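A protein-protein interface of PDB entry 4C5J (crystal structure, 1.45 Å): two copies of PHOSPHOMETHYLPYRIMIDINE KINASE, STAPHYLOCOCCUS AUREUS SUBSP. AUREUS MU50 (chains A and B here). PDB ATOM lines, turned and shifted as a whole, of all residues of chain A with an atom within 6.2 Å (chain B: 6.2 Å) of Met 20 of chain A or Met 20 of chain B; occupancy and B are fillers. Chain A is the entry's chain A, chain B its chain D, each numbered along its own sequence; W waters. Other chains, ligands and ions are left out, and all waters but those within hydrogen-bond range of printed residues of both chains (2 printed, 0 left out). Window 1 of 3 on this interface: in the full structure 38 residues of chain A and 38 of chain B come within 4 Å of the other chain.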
ATOM      1  N   THR A   8       9.744 -10.845 -28.603  1.00  0.00           N
ATOM      2  CA  THR A   8       8.324 -10.629 -28.350  1.00  0.00           C
ATOM      3  C   THR A   8       7.672 -10.046 -29.629  1.00  0.00           C
ATOM      4  O   THR A   8       8.237  -9.202 -30.327  1.00  0.00           O
ATOM      5  CB  THR A   8       8.073  -9.714 -27.159  1.00  0.00           C
ATOM      6  OG1 THR A   8       6.672  -9.711 -26.921  1.00  0.00           O
ATOM      7  CG2 THR A   8       8.644  -8.381 -27.269  1.00  0.00           C
ATOM      8  N   ALA A  10       4.501  -7.937 -30.176  1.00  0.00           N
ATOM      9  CA  ALA A  10       3.671  -7.167 -29.236  1.00  0.00           C
ATOM     10  C   ALA A  10       3.628  -5.688 -29.698  1.00  0.00           C
ATOM     11  O   ALA A  10       4.433  -5.287 -30.517  1.00  0.00           O
ATOM     12  CB  ALA A  10       4.176  -7.267 -27.780  1.00  0.00           C
ATOM     13  N   GLY A  11       2.703  -4.911 -29.133  1.00  0.00           N
ATOM     14  CA  GLY A  11       2.622  -3.524 -29.390  1.00  0.00           C
ATOM     15  C   GLY A  11       3.306  -2.699 -28.315  1.00  0.00           C
ATOM     16  O   GLY A  11       3.731  -3.223 -27.271  1.00  0.00           O
ATOM     17  N   SER A  12       3.427  -1.430 -28.610  1.00  0.00           N
ATOM     18  CA  SER A  12       4.016  -0.491 -27.686  1.00  0.00           C
ATOM     19  C   SER A  12       2.996   0.109 -26.800  1.00  0.00           C
ATOM     20  O   SER A  12       2.031   0.676 -27.282  1.00  0.00           O
ATOM     21  CB  SER A  12       4.785   0.656 -28.430  1.00  0.00           C
ATOM     22  OG  SER A  12       5.267   1.576 -27.526  1.00  0.00           O
ATOM     23  N   ASP A  13       3.180  -0.072 -25.501  1.00  0.00           N
ATOM     24  CA  ASP A  13       2.435   0.577 -24.419  1.00  0.00           C
ATOM     25  C   ASP A  13       3.117   1.855 -24.085  1.00  0.00           C
ATOM     26  O   ASP A  13       4.133   1.805 -23.390  1.00  0.00           O
ATOM     27  CB  ASP A  13       2.308  -0.338 -23.151  1.00  0.00           C
ATOM     28  CG  ASP A  13       1.812   0.418 -21.939  1.00  0.00           C
ATOM     29  OD1 ASP A  13       1.197   1.535 -22.073  1.00  0.00           O
ATOM     30  OD2 ASP A  13       1.937  -0.134 -20.812  1.00  0.00           O
ATOM     31  N   ALA A  18       3.289  -2.155 -19.572  1.00  0.00           N
ATOM     32  CA  ALA A  18       2.881  -3.404 -20.207  1.00  0.00           C
ATOM     33  C   ALA A  18       3.460  -3.461 -21.634  1.00  0.00           C
ATOM     34  O   ALA A  18       4.484  -2.811 -21.965  1.00  0.00           O
ATOM     35  CB  ALA A  18       1.340  -3.512 -20.169  1.00  0.00           C
ATOM     36  N   GLY A  19       2.810  -4.190 -22.546  1.00  0.00           N
ATOM     37  CA  GLY A  19       3.238  -4.242 -23.867  1.00  0.00           C
ATOM     38  C   GLY A  19       4.677  -4.753 -24.077  1.00  0.00           C
ATOM     39  O   GLY A  19       5.226  -5.457 -23.220  1.00  0.00           O
ATOM     40  N   MET A  20       5.287  -4.351 -25.145  1.00  0.00           N
ATOM     41  CA  MET A  20       6.638  -4.717 -25.450  1.00  0.00           C
ATOM     42  C   MET A  20       7.603  -4.168 -24.412  1.00  0.00           C
ATOM     43  O   MET A  20       8.693  -4.733 -24.235  1.00  0.00           O
ATOM     44  CB  MET A  20       7.017  -4.316 -26.827  1.00  0.00           C
ATOM     45  CG  MET A  20       7.085  -2.853 -27.148  1.00  0.00           C
ATOM     46  SD  MET A  20       8.774  -2.157 -26.912  1.00  0.00           S
ATOM     47  CE  MET A  20       8.462  -0.457 -27.434  1.00  0.00           C
ATOM     48  N   GLN A  21       7.269  -3.026 -23.811  1.00  0.00           N
ATOM     49  CA  GLN A  21       8.127  -2.417 -22.833  1.00  0.00           C
ATOM     50  C   GLN A  21       8.306  -3.383 -21.637  1.00  0.00           C
ATOM     51  O   GLN A  21       9.439  -3.640 -21.196  1.00  0.00           O
ATOM     52  CB  GLN A  21       7.539  -1.097 -22.307  1.00  0.00           C
ATOM     53  CG  GLN A  21       7.721   0.053 -23.318  1.00  0.00           C
ATOM     54  CD  GLN A  21       6.640   0.172 -24.370  1.00  0.00           C
ATOM     55  OE1 GLN A  21       5.903  -0.801 -24.686  1.00  0.00           O
ATOM     56  NE2 GLN A  21       6.621   1.336 -25.023  1.00  0.00           N
ATOM     57  N   ALA A  22       7.193  -3.937 -21.152  1.00  0.00           N
ATOM     58  CA  ALA A  22       7.313  -4.921 -20.036  1.00  0.00           C
ATOM     59  C   ALA A  22       8.167  -6.068 -20.489  1.00  0.00           C
ATOM     60  O   ALA A  22       8.975  -6.615 -19.674  1.00  0.00           O
ATOM     61  CB  ALA A  22       5.947  -5.430 -19.621  1.00  0.00           C
ATOM     62  N   ASP A  23       7.974  -6.548 -21.698  1.00  0.00           N
ATOM     63  CA  ASP A  23       8.701  -7.690 -22.265  1.00  0.00           C
ATOM     64  C   ASP A  23      10.204  -7.402 -22.304  1.00  0.00           C
ATOM     65  O   ASP A  23      11.025  -8.163 -21.759  1.00  0.00           O
ATOM     66  CB  ASP A  23       8.185  -8.093 -23.610  1.00  0.00           C
ATOM     67  CG  ASP A  23       6.748  -8.533 -23.623  1.00  0.00           C
ATOM     68  OD1 ASP A  23       6.231  -8.955 -22.547  1.00  0.00           O
ATOM     69  OD2 ASP A  23       6.121  -8.405 -24.728  1.00  0.00           O
ATOM     70  N   LEU A  24      10.617  -6.310 -22.927  1.00  0.00           N
ATOM     71  CA  LEU A  24      12.079  -6.000 -23.018  1.00  0.00           C
ATOM     72  C   LEU A  24      12.696  -5.789 -21.655  1.00  0.00           C
ATOM     73  O   LEU A  24      13.854  -6.171 -21.435  1.00  0.00           O
ATOM     74  CB  LEU A  24      12.282  -4.745 -23.918  1.00  0.00           C
ATOM     75  CG  LEU A  24      11.976  -4.911 -25.411  1.00  0.00           C
ATOM     76  CD1 LEU A  24      12.285  -3.587 -26.116  1.00  0.00           C
ATOM     77  CD2 LEU A  24      12.688  -6.081 -26.103  1.00  0.00           C
ATOM     78  N   LYS A  25      11.974  -5.085 -20.778  1.00  0.00           N
ATOM     79  CA  LYS A  25      12.491  -4.867 -19.453  1.00  0.00           C
ATOM     80  C   LYS A  25      12.733  -6.176 -18.695  1.00  0.00           C
ATOM     81  O   LYS A  25      13.758  -6.360 -18.022  1.00  0.00           O
ATOM     82  CB  LYS A  25      11.588  -3.917 -18.662  1.00  0.00           C
ATOM     83  CG  LYS A  25      11.504  -2.508 -19.255  1.00  0.00           C
ATOM     84  CD  LYS A  25      10.439  -1.671 -18.611  1.00  0.00           C
ATOM     85  CE  LYS A  25      10.396  -0.216 -19.161  1.00  0.00           C
ATOM     86  NZ  LYS A  25       9.528   0.654 -18.378  1.00  0.00           N
ATOM     87  N   VAL A  36      11.948  -7.120 -30.299  1.00  0.00           N
ATOM     88  CA  VAL A  36      10.533  -6.873 -30.493  1.00  0.00           C
ATOM     89  C   VAL A  36      10.274  -6.745 -31.957  1.00  0.00           C
ATOM     90  O   VAL A  36      11.007  -6.077 -32.692  1.00  0.00           O
ATOM     91  CB  VAL A  36      10.012  -5.681 -29.706  1.00  0.00           C
ATOM     92  CG1 VAL A  36      10.824  -4.414 -29.907  1.00  0.00           C
ATOM     93  CG2 VAL A  36       8.537  -5.436 -29.979  1.00  0.00           C
ATOM     94  N   LEU A  38       7.196  -5.011 -33.515  1.00  0.00           N
ATOM     95  CA  LEU A  38       6.108  -4.150 -33.126  1.00  0.00           C
ATOM     96  C   LEU A  38       4.886  -4.298 -34.054  1.00  0.00           C
ATOM     97  O   LEU A  38       4.993  -4.189 -35.237  1.00  0.00           O
ATOM     98  CB  LEU A  38       6.539  -2.673 -33.117  1.00  0.00           C
ATOM     99  CG  LEU A  38       7.682  -2.297 -32.189  1.00  0.00           C
ATOM    100  CD1 LEU A  38       8.330  -1.015 -32.635  1.00  0.00           C
ATOM    101  CD2 LEU A  38       7.172  -2.248 -30.743  1.00  0.00           C
ATOM    102  N   CYS A 214       1.848  -9.399 -18.833  1.00  0.00           N
ATOM    103  CA  CYS A 214       2.903  -9.394 -19.803  1.00  0.00           C
ATOM    104  C   CYS A 214       4.213  -9.853 -19.176  1.00  0.00           C
ATOM    105  O   CYS A 214       4.973 -10.613 -19.765  1.00  0.00           O
ATOM    106  CB  CYS A 214       3.081  -7.981 -20.341  1.00  0.00           C
ATOM    107  SG  CYS A 214       1.714  -7.370 -21.365  1.00  0.00           S
ATOM    108  N   THR B   8      13.137   8.373 -23.641  1.00  0.00           N
ATOM    109  CA  THR B   8      13.886   8.493 -24.875  1.00  0.00           C
ATOM    110  C   THR B   8      12.967   8.821 -26.040  1.00  0.00           C
ATOM    111  O   THR B   8      11.868   8.254 -26.156  1.00  0.00           O
ATOM    112  CB  THR B   8      14.759   7.273 -25.180  1.00  0.00           C
ATOM    113  OG1 THR B   8      15.527   7.594 -26.337  1.00  0.00           O
ATOM    114  CG2 THR B   8      13.973   6.043 -25.486  1.00  0.00           C
ATOM    115  N   ALA B  10      13.197   8.412 -29.798  1.00  0.00           N
ATOM    116  CA  ALA B  10      14.092   7.600 -30.656  1.00  0.00           C
ATOM    117  C   ALA B  10      13.312   6.618 -31.515  1.00  0.00           C
ATOM    118  O   ALA B  10      12.114   6.411 -31.302  1.00  0.00           O
ATOM    119  CB  ALA B  10      15.097   6.831 -29.751  1.00  0.00           C
ATOM    120  N   GLY B  11      14.001   6.033 -32.442  1.00  0.00           N
ATOM    121  CA  GLY B  11      13.464   5.025 -33.350  1.00  0.00           C
ATOM    122  C   GLY B  11      13.701   3.616 -32.834  1.00  0.00           C
ATOM    123  O   GLY B  11      14.554   3.409 -31.925  1.00  0.00           O
ATOM    124  N   SER B  12      12.959   2.671 -33.415  1.00  0.00           N
ATOM    125  CA  SER B  12      13.161   1.280 -33.138  1.00  0.00           C
ATOM    126  C   SER B  12      14.248   0.677 -34.014  1.00  0.00           C
ATOM    127  O   SER B  12      14.140   0.682 -35.227  1.00  0.00           O
ATOM    128  CB  SER B  12      11.887   0.466 -33.257  1.00  0.00           C
ATOM    129  OG  SER B  12      12.120  -0.882 -32.984  1.00  0.00           O
ATOM    130  N   ASP B  13      15.292   0.084 -33.399  1.00  0.00           N
ATOM    131  CA  ASP B  13      16.279  -0.665 -34.109  1.00  0.00           C
ATOM    132  C   ASP B  13      15.818  -2.101 -34.014  1.00  0.00           C
ATOM    133  O   ASP B  13      16.009  -2.736 -32.961  1.00  0.00           O
ATOM    134  CB  ASP B  13      17.647  -0.525 -33.437  1.00  0.00           C
ATOM    135  CG  ASP B  13      18.659  -1.512 -33.932  1.00  0.00           C
ATOM    136  OD1 ASP B  13      18.436  -2.222 -34.932  1.00  0.00           O
ATOM    137  OD2 ASP B  13      19.752  -1.666 -33.265  1.00  0.00           O
ATOM    138  N   ALA B  18      20.841  -1.039 -30.815  1.00  0.00           N
ATOM    139  CA  ALA B  18      20.865   0.405 -30.735  1.00  0.00           C
ATOM    140  C   ALA B  18      19.434   0.938 -30.600  1.00  0.00           C
ATOM    141  O   ALA B  18      18.521   0.202 -30.202  1.00  0.00           O
ATOM    142  CB  ALA B  18      21.565   0.966 -31.984  1.00  0.00           C
ATOM    143  N   GLY B  19      19.225   2.220 -30.957  1.00  0.00           N
ATOM    144  CA  GLY B  19      17.873   2.732 -30.914  1.00  0.00           C
ATOM    145  C   GLY B  19      17.228   2.762 -29.548  1.00  0.00           C
ATOM    146  O   GLY B  19      17.940   2.706 -28.510  1.00  0.00           O
ATOM    147  N   MET B  20      15.897   2.740 -29.525  1.00  0.00           N
ATOM    148  CA  MET B  20      15.180   2.795 -28.284  1.00  0.00           C
ATOM    149  C   MET B  20      15.449   1.538 -27.466  1.00  0.00           C
ATOM    150  O   MET B  20      15.271   1.538 -26.233  1.00  0.00           O
ATOM    151  CB  MET B  20      13.700   3.019 -28.507  1.00  0.00           C
ATOM    152  CG  MET B  20      12.981   1.908 -29.265  1.00  0.00           C
ATOM    153  SD  MET B  20      12.210   0.702 -28.135  1.00  0.00           S
ATOM    154  CE  MET B  20      11.352  -0.331 -29.306  1.00  0.00           C
ATOM    155  N   GLN B  21      15.787   0.419 -28.178  1.00  0.00           N
ATOM    156  CA  GLN B  21      16.043  -0.855 -27.502  1.00  0.00           C
ATOM    157  C   GLN B  21      17.229  -0.659 -26.577  1.00  0.00           C
ATOM    158  O   GLN B  21      17.183  -1.034 -25.378  1.00  0.00           O
ATOM    159  CB  GLN B  21      16.276  -2.005 -28.473  1.00  0.00           C
ATOM    160  CG  GLN B  21      15.014  -2.525 -29.162  1.00  0.00           C
ATOM    161  CD  GLN B  21      14.580  -1.755 -30.417  1.00  0.00           C
ATOM    162  OE1 GLN B  21      14.986  -0.602 -30.650  1.00  0.00           O
ATOM    163  NE2 GLN B  21      13.688  -2.369 -31.193  1.00  0.00           N
ATOM    164  N   ALA B  22      18.311  -0.125 -27.129  1.00  0.00           N
ATOM    165  CA  ALA B  22      19.498   0.176 -26.280  1.00  0.00           C
ATOM    166  C   ALA B  22      19.132   1.076 -25.086  1.00  0.00           C
ATOM    167  O   ALA B  22      19.568   0.859 -23.972  1.00  0.00           O
ATOM    168  CB  ALA B  22      20.663   0.794 -27.049  1.00  0.00           C
ATOM    169  N   ASP B  23      18.327   2.112 -25.356  1.00  0.00           N
ATOM    170  CA  ASP B  23      17.944   3.061 -24.350  1.00  0.00           C
ATOM    171  C   ASP B  23      17.141   2.320 -23.230  1.00  0.00           C
ATOM    172  O   ASP B  23      17.493   2.470 -22.039  1.00  0.00           O
ATOM    173  CB  ASP B  23      17.111   4.139 -24.972  1.00  0.00           C
ATOM    174  CG  ASP B  23      17.874   4.977 -25.968  1.00  0.00           C
ATOM    175  OD1 ASP B  23      19.126   5.046 -25.922  1.00  0.00           O
ATOM    176  OD2 ASP B  23      17.220   5.578 -26.899  1.00  0.00           O
ATOM    177  N   LEU B  24      16.053   1.601 -23.603  1.00  0.00           N
ATOM    178  CA  LEU B  24      15.264   0.960 -22.556  1.00  0.00           C
ATOM    179  C   LEU B  24      16.093  -0.069 -21.773  1.00  0.00           C
ATOM    180  O   LEU B  24      15.919  -0.160 -20.554  1.00  0.00           O
ATOM    181  CB  LEU B  24      14.003   0.300 -23.115  1.00  0.00           C
ATOM    182  CG  LEU B  24      12.964   1.226 -23.754  1.00  0.00           C
ATOM    183  CD1 LEU B  24      11.818   0.394 -24.336  1.00  0.00           C
ATOM    184  CD2 LEU B  24      12.414   2.260 -22.786  1.00  0.00           C
ATOM    185  N   LYS B  25      16.941  -0.793 -22.456  1.00  0.00           N
ATOM    186  CA  LYS B  25      17.751  -1.828 -21.782  1.00  0.00           C
ATOM    187  C   LYS B  25      18.691  -1.176 -20.770  1.00  0.00           C
ATOM    188  O   LYS B  25      18.895  -1.648 -19.670  1.00  0.00           O
ATOM    189  CB  LYS B  25      18.514  -2.674 -22.804  1.00  0.00           C
ATOM    190  CG  LYS B  25      17.631  -3.534 -23.699  1.00  0.00           C
ATOM    191  CD  LYS B  25      18.338  -4.168 -24.841  1.00  0.00           C
ATOM    192  CE  LYS B  25      17.441  -5.035 -25.673  1.00  0.00           C
ATOM    193  NZ  LYS B  25      18.218  -5.861 -26.555  1.00  0.00           N
ATOM    194  N   VAL B  36       9.534   5.353 -23.931  1.00  0.00           N
ATOM    195  CA  VAL B  36       9.968   5.763 -25.245  1.00  0.00           C
ATOM    196  C   VAL B  36       8.772   6.422 -26.002  1.00  0.00           C
ATOM    197  O   VAL B  36       7.608   6.010 -25.898  1.00  0.00           O
ATOM    198  CB  VAL B  36      10.424   4.565 -26.103  1.00  0.00           C
ATOM    199  CG1 VAL B  36       9.459   3.388 -26.070  1.00  0.00           C
ATOM    200  CG2 VAL B  36      10.810   4.930 -27.529  1.00  0.00           C
ATOM    201  N   LEU B  38       8.304   6.779 -29.888  1.00  0.00           N
ATOM    202  CA  LEU B  38       8.883   6.188 -31.084  1.00  0.00           C
ATOM    203  C   LEU B  38       8.723   7.148 -32.274  1.00  0.00           C
ATOM    204  O   LEU B  38       7.602   7.679 -32.520  1.00  0.00           O
ATOM    205  CB  LEU B  38       8.191   4.878 -31.435  1.00  0.00           C
ATOM    206  CG  LEU B  38       8.361   3.792 -30.397  1.00  0.00           C
ATOM    207  CD1 LEU B  38       7.307   2.714 -30.650  1.00  0.00           C
ATOM    208  CD2 LEU B  38       9.743   3.163 -30.582  1.00  0.00           C
ATOM    209  N   CYS B 214      24.323   5.009 -28.540  1.00  0.00           N
ATOM    210  CA  CYS B 214      22.995   5.094 -27.885  1.00  0.00           C
ATOM    211  C   CYS B 214      23.139   4.740 -26.422  1.00  0.00           C
ATOM    212  O   CYS B 214      22.597   5.408 -25.523  1.00  0.00           O
ATOM    213  CB  CYS B 214      22.023   4.139 -28.528  1.00  0.00           C
ATOM    214  SG  CYS B 214      21.553   4.645 -30.202  1.00  0.00           S
HETATM  215  O   HOH W   1       6.969   4.190 -23.936  1.00  0.00           O
HETATM  216  O   HOH W   2      13.552  -5.317 -31.848  1.00  0.00           O
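Water W1 lies within hydrogen-bond range of O of Val 36 of chain B (2.8 Å) and NE2 of Gln 21 of chain A (3.1 Å). Water W2 lies within hydrogen-bond range of O of Val 36 of chain A and NE2 of Gln 21 of chain B.
Among the printed residues, merely in contact across the chains: Met 20 of chain A with Met 20 of chain B, Gln 21 of chain A with Val 36 of chain B, Val 36 of chain A with Gln 21 of chain B, Leu 38 of chain A with Ser 12 of chain B and Ser 12 of chain A with Leu 38 of chain B.
Ser 12 of chain A touches Leu 38 of chain B, and with the chains exchanged Leu 38 of chain A touches Ser 12 of chain B. Met 20 of chain B touches its own counterpart, Met 20 of chain A. Gln 21 of chain A touches Val 36 of chain B, and with the chains exchanged Val 36 of chain A touches Gln 21 of chain B. Of the 5 pairs that touch across the chains among the printed residues, 5 have their exchanged pair printed and touching as well.
The side-chain hydroxyl of Ser 12 of chain B sits at hydrogen-bond distance from the side-chain amide nitrogen of Gln 21 of chain B (2.8 Å). O of Gly 11 of chain A is in hydrogen-bond range of N of Met 20 of chain A (2.9 Å). The side-chain amide oxygen (OE1) of Gln 21 of chain B lies within hydrogen-bond range of the backbone NH (N) of Asp 13 of chain B, 2.8 Å away. The backbone NH (N) of Met 20 of chain B lies within hydrogen-bond range of the backbone carbonyl oxygen (O) of Gly 11 of chain B (2.8 Å). The side-chain amide oxygen (OE1) of Gln 21 of chain A sits at hydrogen-bond distance from the backbone NH (N) of Asp 13 of chain A. NE2 of Gln 21 of chain A sits at hydrogen-bond distance from OG of Ser 12 of chain A (2.9 Å).
Met 20 of chain A touches just one residue of chain B: Met 20 (3.4 Å). Met 20 of chain B touches just one residue of chain A: Met 20. Of the printed residues of chain B, Gln 21 of chain A touches Val 36. Of the printed residues of chain A, Ser 12 of chain B touches Leu 38 (3.8 Å). Cys 214 of chain B touches none of the printed residues of chain A. Ala 22 of chain B touches none of the printed residues of chain A. The nearest residue of chain B that does not touch Met 20 of chain A is Val 36 of chain B (4.2 Å). The nearest residue of chain A that does not touch Met 20 of chain B is Val 36 of chain A (4.2 Å). The nearest printed residue of chain A that does not touch Gln 21 of chain B is Leu 24 of chain A (4.2 Å).
Of the 16 printed residues of chain A, 5 touch a printed residue of chain B. Printed residues of chain A that touch a printed residue of chain B: Ser 12, Met 20, Gln 21, Val 36 and Leu 38. Of the 16 printed residues of chain B, 5 touch a printed residue of chain A. Among the printed residues, 5 pairs touch across the chains.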
